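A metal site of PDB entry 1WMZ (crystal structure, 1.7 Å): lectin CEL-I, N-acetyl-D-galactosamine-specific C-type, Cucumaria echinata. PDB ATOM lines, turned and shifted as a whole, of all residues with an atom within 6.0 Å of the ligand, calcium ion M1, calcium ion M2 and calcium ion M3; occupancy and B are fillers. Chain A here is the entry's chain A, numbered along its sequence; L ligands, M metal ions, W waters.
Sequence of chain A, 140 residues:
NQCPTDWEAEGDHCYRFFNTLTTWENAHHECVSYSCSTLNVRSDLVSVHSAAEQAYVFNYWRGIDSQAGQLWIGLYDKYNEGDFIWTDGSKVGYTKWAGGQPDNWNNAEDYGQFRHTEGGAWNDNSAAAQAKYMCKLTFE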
ATOM      1  N   GLN A  70      17.540 -39.203   1.936  1.00  0.00           N
ATOM      2  CA  GLN A  70      17.765 -37.760   1.871  1.00  0.00           C
ATOM      3  C   GLN A  70      18.946 -37.310   2.753  1.00  0.00           C
ATOM      4  O   GLN A  70      19.438 -38.068   3.585  1.00  0.00           O
ATOM      5  CB  GLN A  70      16.497 -37.045   2.312  1.00  0.00           C
ATOM      6  CG  GLN A  70      15.361 -37.237   1.266  1.00  0.00           C
ATOM      7  CD  GLN A  70      14.615 -38.573   1.443  1.00  0.00           C
ATOM      8  OE1 GLN A  70      14.090 -38.874   2.498  1.00  0.00           O
ATOM      9  NE2 GLN A  70      14.541 -39.341   0.376  1.00  0.00           N
ATOM     10  N   ASP A  77      12.036 -23.010   7.236  1.00  0.00           N
ATOM     11  CA  ASP A  77      11.025 -21.958   7.285  1.00  0.00           C
ATOM     12  C   ASP A  77      10.149 -22.096   8.544  1.00  0.00           C
ATOM     13  O   ASP A  77       8.976 -21.704   8.547  1.00  0.00           O
ATOM     14  CB  ASP A  77      10.185 -21.949   6.002  1.00  0.00           C
ATOM     15  CG  ASP A  77       9.084 -22.983   6.006  1.00  0.00           C
ATOM     16  OD1 ASP A  77       9.244 -24.058   6.633  1.00  0.00           O
ATOM     17  OD2 ASP A  77       7.991 -22.790   5.410  1.00  0.00           O
ATOM     18  N   LYS A  78      10.729 -22.639   9.615  1.00  0.00           N
ATOM     19  CA  LYS A  78      10.056 -22.817  10.915  1.00  0.00           C
ATOM     20  C   LYS A  78       9.537 -21.499  11.489  1.00  0.00           C
ATOM     21  O   LYS A  78       8.404 -21.443  12.005  1.00  0.00           O
ATOM     22  CB  LYS A  78      11.024 -23.432  11.933  1.00  0.00           C
ATOM     23  CG  LYS A  78      10.396 -23.757  13.290  1.00  0.00           C
ATOM     24  CD  LYS A  78      11.397 -23.520  14.398  1.00  0.00           C
ATOM     25  CE  LYS A  78      10.871 -23.934  15.776  1.00  0.00           C
ATOM     26  NZ  LYS A  78      11.316 -25.324  16.187  1.00  0.00           N
ATOM     27  N   GLU A  81       6.571 -19.266   7.980  1.00  0.00           N
ATOM     28  CA  GLU A  81       6.092 -20.194   6.938  1.00  0.00           C
ATOM     29  C   GLU A  81       6.199 -19.616   5.538  1.00  0.00           C
ATOM     30  O   GLU A  81       5.704 -18.505   5.254  1.00  0.00           O
ATOM     31  CB  GLU A  81       4.659 -20.636   7.234  1.00  0.00           C
ATOM     32  CG  GLU A  81       4.095 -21.687   6.242  1.00  0.00           C
ATOM     33  CD  GLU A  81       4.951 -22.944   6.076  1.00  0.00           C
ATOM     34  OE1 GLU A  81       5.107 -23.418   4.940  1.00  0.00           O
ATOM     35  OE2 GLU A  81       5.445 -23.467   7.085  1.00  0.00           O
ATOM     36  N   GLY A  82       6.871 -20.385   4.673  1.00  0.00           N
ATOM     37  CA  GLY A  82       7.116 -20.047   3.287  1.00  0.00           C
ATOM     38  C   GLY A  82       8.366 -19.265   2.968  1.00  0.00           C
ATOM     39  O   GLY A  82       8.750 -19.182   1.812  1.00  0.00           O
ATOM     40  N   PHE A  84      12.049 -19.438   3.351  1.00  0.00           N
ATOM     41  CA  PHE A  84      13.170 -20.336   3.647  1.00  0.00           C
ATOM     42  C   PHE A  84      14.447 -19.536   3.835  1.00  0.00           C
ATOM     43  O   PHE A  84      14.737 -18.612   3.044  1.00  0.00           O
ATOM     44  CB  PHE A  84      13.295 -21.424   2.588  1.00  0.00           C
ATOM     45  CG  PHE A  84      12.314 -22.551   2.809  1.00  0.00           C
ATOM     46  CD1 PHE A  84      12.638 -23.599   3.645  1.00  0.00           C
ATOM     47  CD2 PHE A  84      11.055 -22.522   2.192  1.00  0.00           C
ATOM     48  CE1 PHE A  84      11.779 -24.635   3.877  1.00  0.00           C
ATOM     49  CE2 PHE A  84      10.156 -23.564   2.414  1.00  0.00           C
ATOM     50  CZ  PHE A  84      10.503 -24.623   3.267  1.00  0.00           C
ATOM     51  N   GLY A 100       7.453 -29.431  -7.751  1.00  0.00           N
ATOM     52  CA  GLY A 100       6.355 -29.564  -6.781  1.00  0.00           C
ATOM     53  C   GLY A 100       6.700 -29.192  -5.347  1.00  0.00           C
ATOM     54  O   GLY A 100       5.844 -29.298  -4.445  1.00  0.00           O
ATOM     55  N   GLN A 101       7.947 -28.743  -5.160  1.00  0.00           N
ATOM     56  CA  GLN A 101       8.484 -28.387  -3.834  1.00  0.00           C
ATOM     57  C   GLN A 101       8.960 -26.928  -3.823  1.00  0.00           C
ATOM     58  O   GLN A 101       9.380 -26.398  -4.866  1.00  0.00           O
ATOM     59  CB  GLN A 101       9.682 -29.305  -3.517  1.00  0.00           C
ATOM     60  CG  GLN A 101       9.368 -30.798  -3.567  1.00  0.00           C
ATOM     61  CD  GLN A 101       8.281 -31.237  -2.608  1.00  0.00           C
ATOM     62  OE1 GLN A 101       7.981 -30.567  -1.656  1.00  0.00           O
ATOM     63  NE2 GLN A 101       7.652 -32.374  -2.901  1.00  0.00           N
ATOM     64  N   PRO A 102       8.925 -26.266  -2.678  1.00  0.00           N
ATOM     65  CA  PRO A 102       8.425 -26.783  -1.396  1.00  0.00           C
ATOM     66  C   PRO A 102       6.900 -26.727  -1.352  1.00  0.00           C
ATOM     67  O   PRO A 102       6.295 -25.894  -2.030  1.00  0.00           O
ATOM     68  CB  PRO A 102       8.998 -25.769  -0.385  1.00  0.00           C
ATOM     69  CG  PRO A 102       8.990 -24.505  -1.119  1.00  0.00           C
ATOM     70  CD  PRO A 102       9.328 -24.855  -2.541  1.00  0.00           C
ATOM     71  N   ASP A 103       6.294 -27.576  -0.564  1.00  0.00           N
ATOM     72  CA  ASP A 103       4.818 -27.727  -0.543  1.00  0.00           C
ATOM     73  C   ASP A 103       4.196 -27.734   0.838  1.00  0.00           C
ATOM     74  O   ASP A 103       3.001 -27.861   0.966  1.00  0.00           O
ATOM     75  CB  ASP A 103       4.390 -28.975  -1.350  1.00  0.00           C
ATOM     76  CG  ASP A 103       4.868 -30.264  -0.721  1.00  0.00           C
ATOM     77  OD1 ASP A 103       4.444 -31.386  -1.177  1.00  0.00           O
ATOM     78  OD2 ASP A 103       5.684 -30.273   0.238  1.00  0.00           O
ATOM     79  N   ASN A 104       4.986 -27.597   1.895  1.00  0.00           N
ATOM     80  CA  ASN A 104       4.484 -27.635   3.260  1.00  0.00           C
ATOM     81  C   ASN A 104       3.448 -28.749   3.498  1.00  0.00           C
ATOM     82  O   ASN A 104       2.407 -28.523   4.092  1.00  0.00           O
ATOM     83  CB  ASN A 104       3.904 -26.259   3.636  1.00  0.00           C
ATOM     84  CG  ASN A 104       3.806 -26.055   5.126  1.00  0.00           C
ATOM     85  OD1 ASN A 104       4.747 -26.319   5.897  1.00  0.00           O
ATOM     86  ND2 ASN A 104       2.668 -25.541   5.552  1.00  0.00           N
ATOM     87  N   TRP A 105       3.761 -29.944   3.024  1.00  0.00           N
ATOM     88  CA  TRP A 105       2.818 -31.043   3.084  1.00  0.00           C
ATOM     89  C   TRP A 105       2.329 -31.268   4.506  1.00  0.00           C
ATOM     90  O   TRP A 105       3.108 -31.296   5.462  1.00  0.00           O
ATOM     91  CB  TRP A 105       3.504 -32.285   2.534  1.00  0.00           C
ATOM     92  CG  TRP A 105       2.646 -33.467   2.376  1.00  0.00           C
ATOM     93  CD1 TRP A 105       1.693 -33.665   1.455  1.00  0.00           C
ATOM     94  CD2 TRP A 105       2.733 -34.679   3.143  1.00  0.00           C
ATOM     95  NE1 TRP A 105       1.168 -34.927   1.569  1.00  0.00           N
ATOM     96  CE2 TRP A 105       1.769 -35.557   2.623  1.00  0.00           C
ATOM     97  CE3 TRP A 105       3.499 -35.097   4.232  1.00  0.00           C
ATOM     98  CZ2 TRP A 105       1.568 -36.837   3.144  1.00  0.00           C
ATOM     99  CZ3 TRP A 105       3.305 -36.365   4.756  1.00  0.00           C
ATOM    100  CH2 TRP A 105       2.326 -37.218   4.213  1.00  0.00           C
ATOM    101  N   ASN A 107       0.979 -29.325   6.340  1.00  0.00           N
ATOM    102  CA  ASN A 107       1.318 -28.133   7.156  1.00  0.00           C
ATOM    103  C   ASN A 107       2.418 -28.350   8.174  1.00  0.00           C
ATOM    104  O   ASN A 107       2.488 -27.644   9.159  1.00  0.00           O
ATOM    105  CB  ASN A 107       0.063 -27.627   7.857  1.00  0.00           C
ATOM    106  CG  ASN A 107      -1.051 -27.312   6.891  1.00  0.00           C
ATOM    107  OD1 ASN A 107      -0.900 -26.442   5.997  1.00  0.00           O
ATOM    108  ND2 ASN A 107      -2.190 -27.984   7.050  1.00  0.00           N
ATOM    109  N   ALA A 108       3.321 -29.277   7.918  1.00  0.00           N
ATOM    110  CA  ALA A 108       4.317 -29.662   8.910  1.00  0.00           C
ATOM    111  C   ALA A 108       5.739 -29.803   8.343  1.00  0.00           C
ATOM    112  O   ALA A 108       6.642 -30.328   9.026  1.00  0.00           O
ATOM    113  CB  ALA A 108       3.892 -30.919   9.596  1.00  0.00           C
ATOM    114  N   GLU A 109       5.962 -29.338   7.113  1.00  0.00           N
ATOM    115  CA  GLU A 109       7.265 -29.450   6.498  1.00  0.00           C
ATOM    116  C   GLU A 109       7.991 -28.084   6.447  1.00  0.00           C
ATOM    117  O   GLU A 109       7.644 -27.200   5.635  1.00  0.00           O
ATOM    118  CB  GLU A 109       7.186 -30.080   5.096  1.00  0.00           C
ATOM    119  CG  GLU A 109       6.455 -31.421   5.061  1.00  0.00           C
ATOM    120  CD  GLU A 109       6.664 -32.149   3.782  1.00  0.00           C
ATOM    121  OE1 GLU A 109       6.688 -31.512   2.708  1.00  0.00           O
ATOM    122  OE2 GLU A 109       6.818 -33.412   3.808  1.00  0.00           O
ATOM    123  N   ASP A 110       9.014 -27.962   7.289  1.00  0.00           N
ATOM    124  CA  ASP A 110       9.807 -26.721   7.447  1.00  0.00           C
ATOM    125  C   ASP A 110      11.331 -26.896   7.335  1.00  0.00           C
ATOM    126  O   ASP A 110      12.071 -25.967   7.621  1.00  0.00           O
ATOM    127  CB  ASP A 110       9.532 -26.110   8.809  1.00  0.00           C
ATOM    128  CG  ASP A 110       8.043 -26.058   9.164  1.00  0.00           C
ATOM    129  OD1 ASP A 110       7.732 -26.364  10.333  1.00  0.00           O
ATOM    130  OD2 ASP A 110       7.118 -25.732   8.380  1.00  0.00           O
ATOM    131  N   TYR A 111      11.789 -28.061   6.946  1.00  0.00           N
ATOM    132  CA  TYR A 111      13.202 -28.434   7.031  1.00  0.00           C
ATOM    133  C   TYR A 111      13.694 -28.967   5.692  1.00  0.00           C
ATOM    134  O   TYR A 111      13.187 -29.951   5.147  1.00  0.00           O
ATOM    135  CB  TYR A 111      13.335 -29.484   8.170  1.00  0.00           C
ATOM    136  CG  TYR A 111      12.701 -28.996   9.440  1.00  0.00           C
ATOM    137  CD1 TYR A 111      11.481 -29.527   9.907  1.00  0.00           C
ATOM    138  CD2 TYR A 111      13.259 -27.938  10.131  1.00  0.00           C
ATOM    139  CE1 TYR A 111      10.890 -29.042  11.080  1.00  0.00           C
ATOM    140  CE2 TYR A 111      12.689 -27.451  11.282  1.00  0.00           C
ATOM    141  CZ  TYR A 111      11.494 -28.002  11.763  1.00  0.00           C
ATOM    142  OH  TYR A 111      10.915 -27.476  12.885  1.00  0.00           O
ATOM    143  N   GLN A 113      16.219 -30.430   2.634  1.00  0.00           N
ATOM    144  CA  GLN A 113      17.023 -31.636   2.435  1.00  0.00           C
ATOM    145  C   GLN A 113      17.189 -31.908   0.941  1.00  0.00           C
ATOM    146  O   GLN A 113      16.297 -31.589   0.132  1.00  0.00           O
ATOM    147  CB  GLN A 113      16.367 -32.834   3.130  1.00  0.00           C
ATOM    148  CG  GLN A 113      14.927 -33.129   2.581  1.00  0.00           C
ATOM    149  CD  GLN A 113      14.213 -34.416   3.137  1.00  0.00           C
ATOM    150  OE1 GLN A 113      13.249 -34.890   2.499  1.00  0.00           O
ATOM    151  NE2 GLN A 113      14.626 -34.909   4.295  1.00  0.00           N
ATOM    152  N   ARG A 115      17.166 -34.602  -1.992  1.00  0.00           N
ATOM    153  CA  ARG A 115      16.888 -35.950  -2.472  1.00  0.00           C
ATOM    154  C   ARG A 115      18.145 -36.656  -2.983  1.00  0.00           C
ATOM    155  O   ARG A 115      19.138 -36.000  -3.337  1.00  0.00           O
ATOM    156  CB  ARG A 115      15.872 -35.904  -3.598  1.00  0.00           C
ATOM    157  CG  ARG A 115      14.521 -35.528  -3.172  1.00  0.00           C
ATOM    158  CD  ARG A 115      13.579 -35.404  -4.320  1.00  0.00           C
ATOM    159  NE  ARG A 115      12.199 -35.213  -3.876  1.00  0.00           N
ATOM    160  CZ  ARG A 115      11.201 -34.925  -4.700  1.00  0.00           C
ATOM    161  NH1 ARG A 115      11.431 -34.788  -6.009  1.00  0.00           N
ATOM    162  NH2 ARG A 115      10.001 -34.713  -4.217  1.00  0.00           N
ATOM    163  N   ASN A 123      13.856 -30.766  -1.175  1.00  0.00           N
ATOM    164  CA  ASN A 123      12.527 -31.013  -0.637  1.00  0.00           C
ATOM    165  C   ASN A 123      12.428 -30.412   0.755  1.00  0.00           C
ATOM    166  O   ASN A 123      13.387 -30.401   1.525  1.00  0.00           O
ATOM    167  CB  ASN A 123      12.261 -32.503  -0.522  1.00  0.00           C
ATOM    168  CG  ASN A 123      10.968 -32.789   0.170  1.00  0.00           C
ATOM    169  OD1 ASN A 123       9.913 -32.291  -0.272  1.00  0.00           O
ATOM    170  ND2 ASN A 123      10.996 -33.606   1.239  1.00  0.00           N
ATOM    171  N   ASP A 124      11.246 -29.919   1.113  1.00  0.00           N
ATOM    172  CA  ASP A 124      10.975 -29.629   2.503  1.00  0.00           C
ATOM    173  C   ASP A 124      10.325 -30.807   3.172  1.00  0.00           C
ATOM    174  O   ASP A 124       9.408 -31.398   2.601  1.00  0.00           O
ATOM    175  CB  ASP A 124      10.096 -28.364   2.662  1.00  0.00           C
ATOM    176  CG  ASP A 124       8.768 -28.467   1.935  1.00  0.00           C
ATOM    177  OD1 ASP A 124       8.662 -29.237   0.953  1.00  0.00           O
ATOM    178  OD2 ASP A 124       7.801 -27.752   2.266  1.00  0.00           O
ATOM    179  N   ASN A 125      10.767 -31.168   4.379  1.00  0.00           N
ATOM    180  CA  ASN A 125      10.227 -32.292   5.133  1.00  0.00           C
ATOM    181  C   ASN A 125       9.983 -31.909   6.623  1.00  0.00           C
ATOM    182  O   ASN A 125      10.264 -30.786   7.033  1.00  0.00           O
ATOM    183  CB  ASN A 125      11.183 -33.494   4.968  1.00  0.00           C
ATOM    184  CG  ASN A 125      10.464 -34.840   4.962  1.00  0.00           C
ATOM    185  OD1 ASN A 125       9.510 -35.045   5.724  1.00  0.00           O
ATOM    186  ND2 ASN A 125      10.951 -35.745   4.180  1.00  0.00           N
HETATM  187  C1  LIG L   1       7.471 -36.234  -1.565  1.00  0.00           C
HETATM  188  C2  LIG L   1       8.201 -35.508  -0.409  1.00  0.00           C
HETATM  189  C3  LIG L   1       7.409 -34.908   0.726  1.00  0.00           C
HETATM  190  C4  LIG L   1       6.022 -34.487   0.340  1.00  0.00           C
HETATM  191  C5  LIG L   1       5.332 -35.255  -0.758  1.00  0.00           C
HETATM  192  C6  LIG L   1       4.035 -34.599  -1.275  1.00  0.00           C
HETATM  193  C7  LIG L   1      10.538 -36.172  -0.461  1.00  0.00           C
HETATM  194  C8  LIG L   1      11.589 -37.020   0.200  1.00  0.00           C
HETATM  195  N1  LIG L   1       9.321 -36.245   0.093  1.00  0.00           N
HETATM  196  O1  LIG L   1       8.201 -36.347  -2.789  1.00  0.00           O
HETATM  197  O2  LIG L   1       8.051 -33.909   1.530  1.00  0.00           O
HETATM  198  O3  LIG L   1       6.250 -33.227  -0.303  1.00  0.00           O
HETATM  199  O4  LIG L   1       6.116 -35.787  -1.808  1.00  0.00           O
HETATM  200  O5  LIG L   1       3.383 -35.647  -2.000  1.00  0.00           O
HETATM  201  O6  LIG L   1      10.788 -35.453  -1.416  1.00  0.00           O
HETATM  202 CA    CA M   1       7.773 -31.502   0.760  1.00  0.00          CA
HETATM  203 CA    CA M   2       6.948 -24.931   5.859  1.00  0.00          CA
HETATM  204 CA    CA M   3       5.690 -24.184   9.533  1.00  0.00          CA
HETATM  205  O   HOH W   1       7.160 -25.459   3.542  1.00  0.00           O
HETATM  206  O   HOH W   2       1.334 -34.944  -3.479  1.00  0.00           O
HETATM  207  O   HOH W   3       6.604 -22.157   9.684  1.00  0.00           O
HETATM  208  O   HOH W   4       2.704 -37.696  -0.307  1.00  0.00           O
HETATM  209  O   HOH W   5       9.034 -38.134   2.401  1.00  0.00           O
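Five residues have an atom within 4 Å of calcium ion M2: Asp 77, Glu 81, Asn 104, Glu 109 and Asp 110. The nearest printed residue that does not touch calcium ion M2 is Phe 84 (4.4 Å).
N of Trp 105 sits close to OE1 of Glu 109 (3.3 Å). The side-chain carboxylate (OD2) of Asp 103 lies close to the backbone NH (N) of Trp 105 (3.4 Å). The side-chain carboxylate of Asp 124 is in hydrogen-bond range of the backbone NH of Asn 104, 2.8 Å away. The side-chain amide nitrogen of Asn 123 is in hydrogen-bond range of the side-chain amide oxygen of Gln 113, 2.9 Å away. The backbone carbonyl oxygen (O) of Asn 125 sits at hydrogen-bond distance from the backbone NH (N) of Asp 110, at 3.1 Å. The side-chain carboxylate of Asp 77 sits close to the backbone NH of Gly 82 (2.8 Å). The side-chain amide oxygen of Gln 113 sits at hydrogen-bond distance from the side-chain amide nitrogen of Asn 125 (3.0 Å).
Calcium ion M3 is bound by water W3 (2.2 Å), the side-chain carboxylate (OD2) of Asp 110 (2.4 Å) and the side-chain carboxylate (OE2) of Glu 81 (2.6 Å). Calcium ion M3 has three donor atoms within binding distance. Slightly farther from calcium ion M3 lies OD1 of Asp 110 (3.1 Å).
Calcium ion M2 is bound by the backbone carbonyl oxygen (O) of Glu 109 (2.4 Å), water W1 (2.4 Å), the side-chain carboxylate (OD2) of Asp 77 (2.4 Å), the side-chain carboxylate (OE2) of Glu 81 (2.4 Å), the side-chain carboxylate (OE1) of Glu 81 (2.6 Å), the side-chain carboxylate (OD1) of Asp 77 (2.6 Å), the side-chain amide oxygen (OD1) of Asn 104 (2.6 Å) and the side-chain carboxylate (OD2) of Asp 110 (2.7 Å). Calcium ion M2 has eight donor atoms within binding distance.
Calcium ion M1 is bound by OE1 of Glu 109 (2.2 Å), OD1 of Asp 124 (2.4 Å), O of Asp 124 (2.5 Å), OD2 of Asp 103 (2.5 Å), OD1 of Asn 123 (2.5 Å), O3 of the ligand (2.5 Å), O2 of the ligand (2.5 Å) and OE1 of Gln 101 (2.6 Å). Calcium ion M1 has eight donor atoms within binding distance.
Water W1 bridges the side-chain carboxylate (OD2) of Asp 124 (2.7 Å) and the backbone NH (N) of Asn 104 (3.5 Å).
O1 of the ligand is in hydrogen-bond range of NH2 of Arg 115 (2.8 Å).
Two residues have an atom within 4 Å of calcium ion M3: Glu 81 and Asp 110. The nearest printed residue that does not touch calcium ion M3 is Asp 77 (4.2 Å).
Residues that only touch the ligand: Gln 113 (3.5 Å), Gln 70 (3.6 Å) and Trp 105 (3.7 Å). Hydrophobic or aromatic side chains within 4 Å of the ligand: Trp 105. Within 4 Å of the ligand: Gln 70, Gln 101, Asp 103, Trp 105, Glu 109, Gln 113, Arg 115, Asn 123 and Asp 124.
Five residues have an atom within 4 Å of calcium ion M1: Gln 101, Asp 103, Glu 109, Asn 123 and Asp 124.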
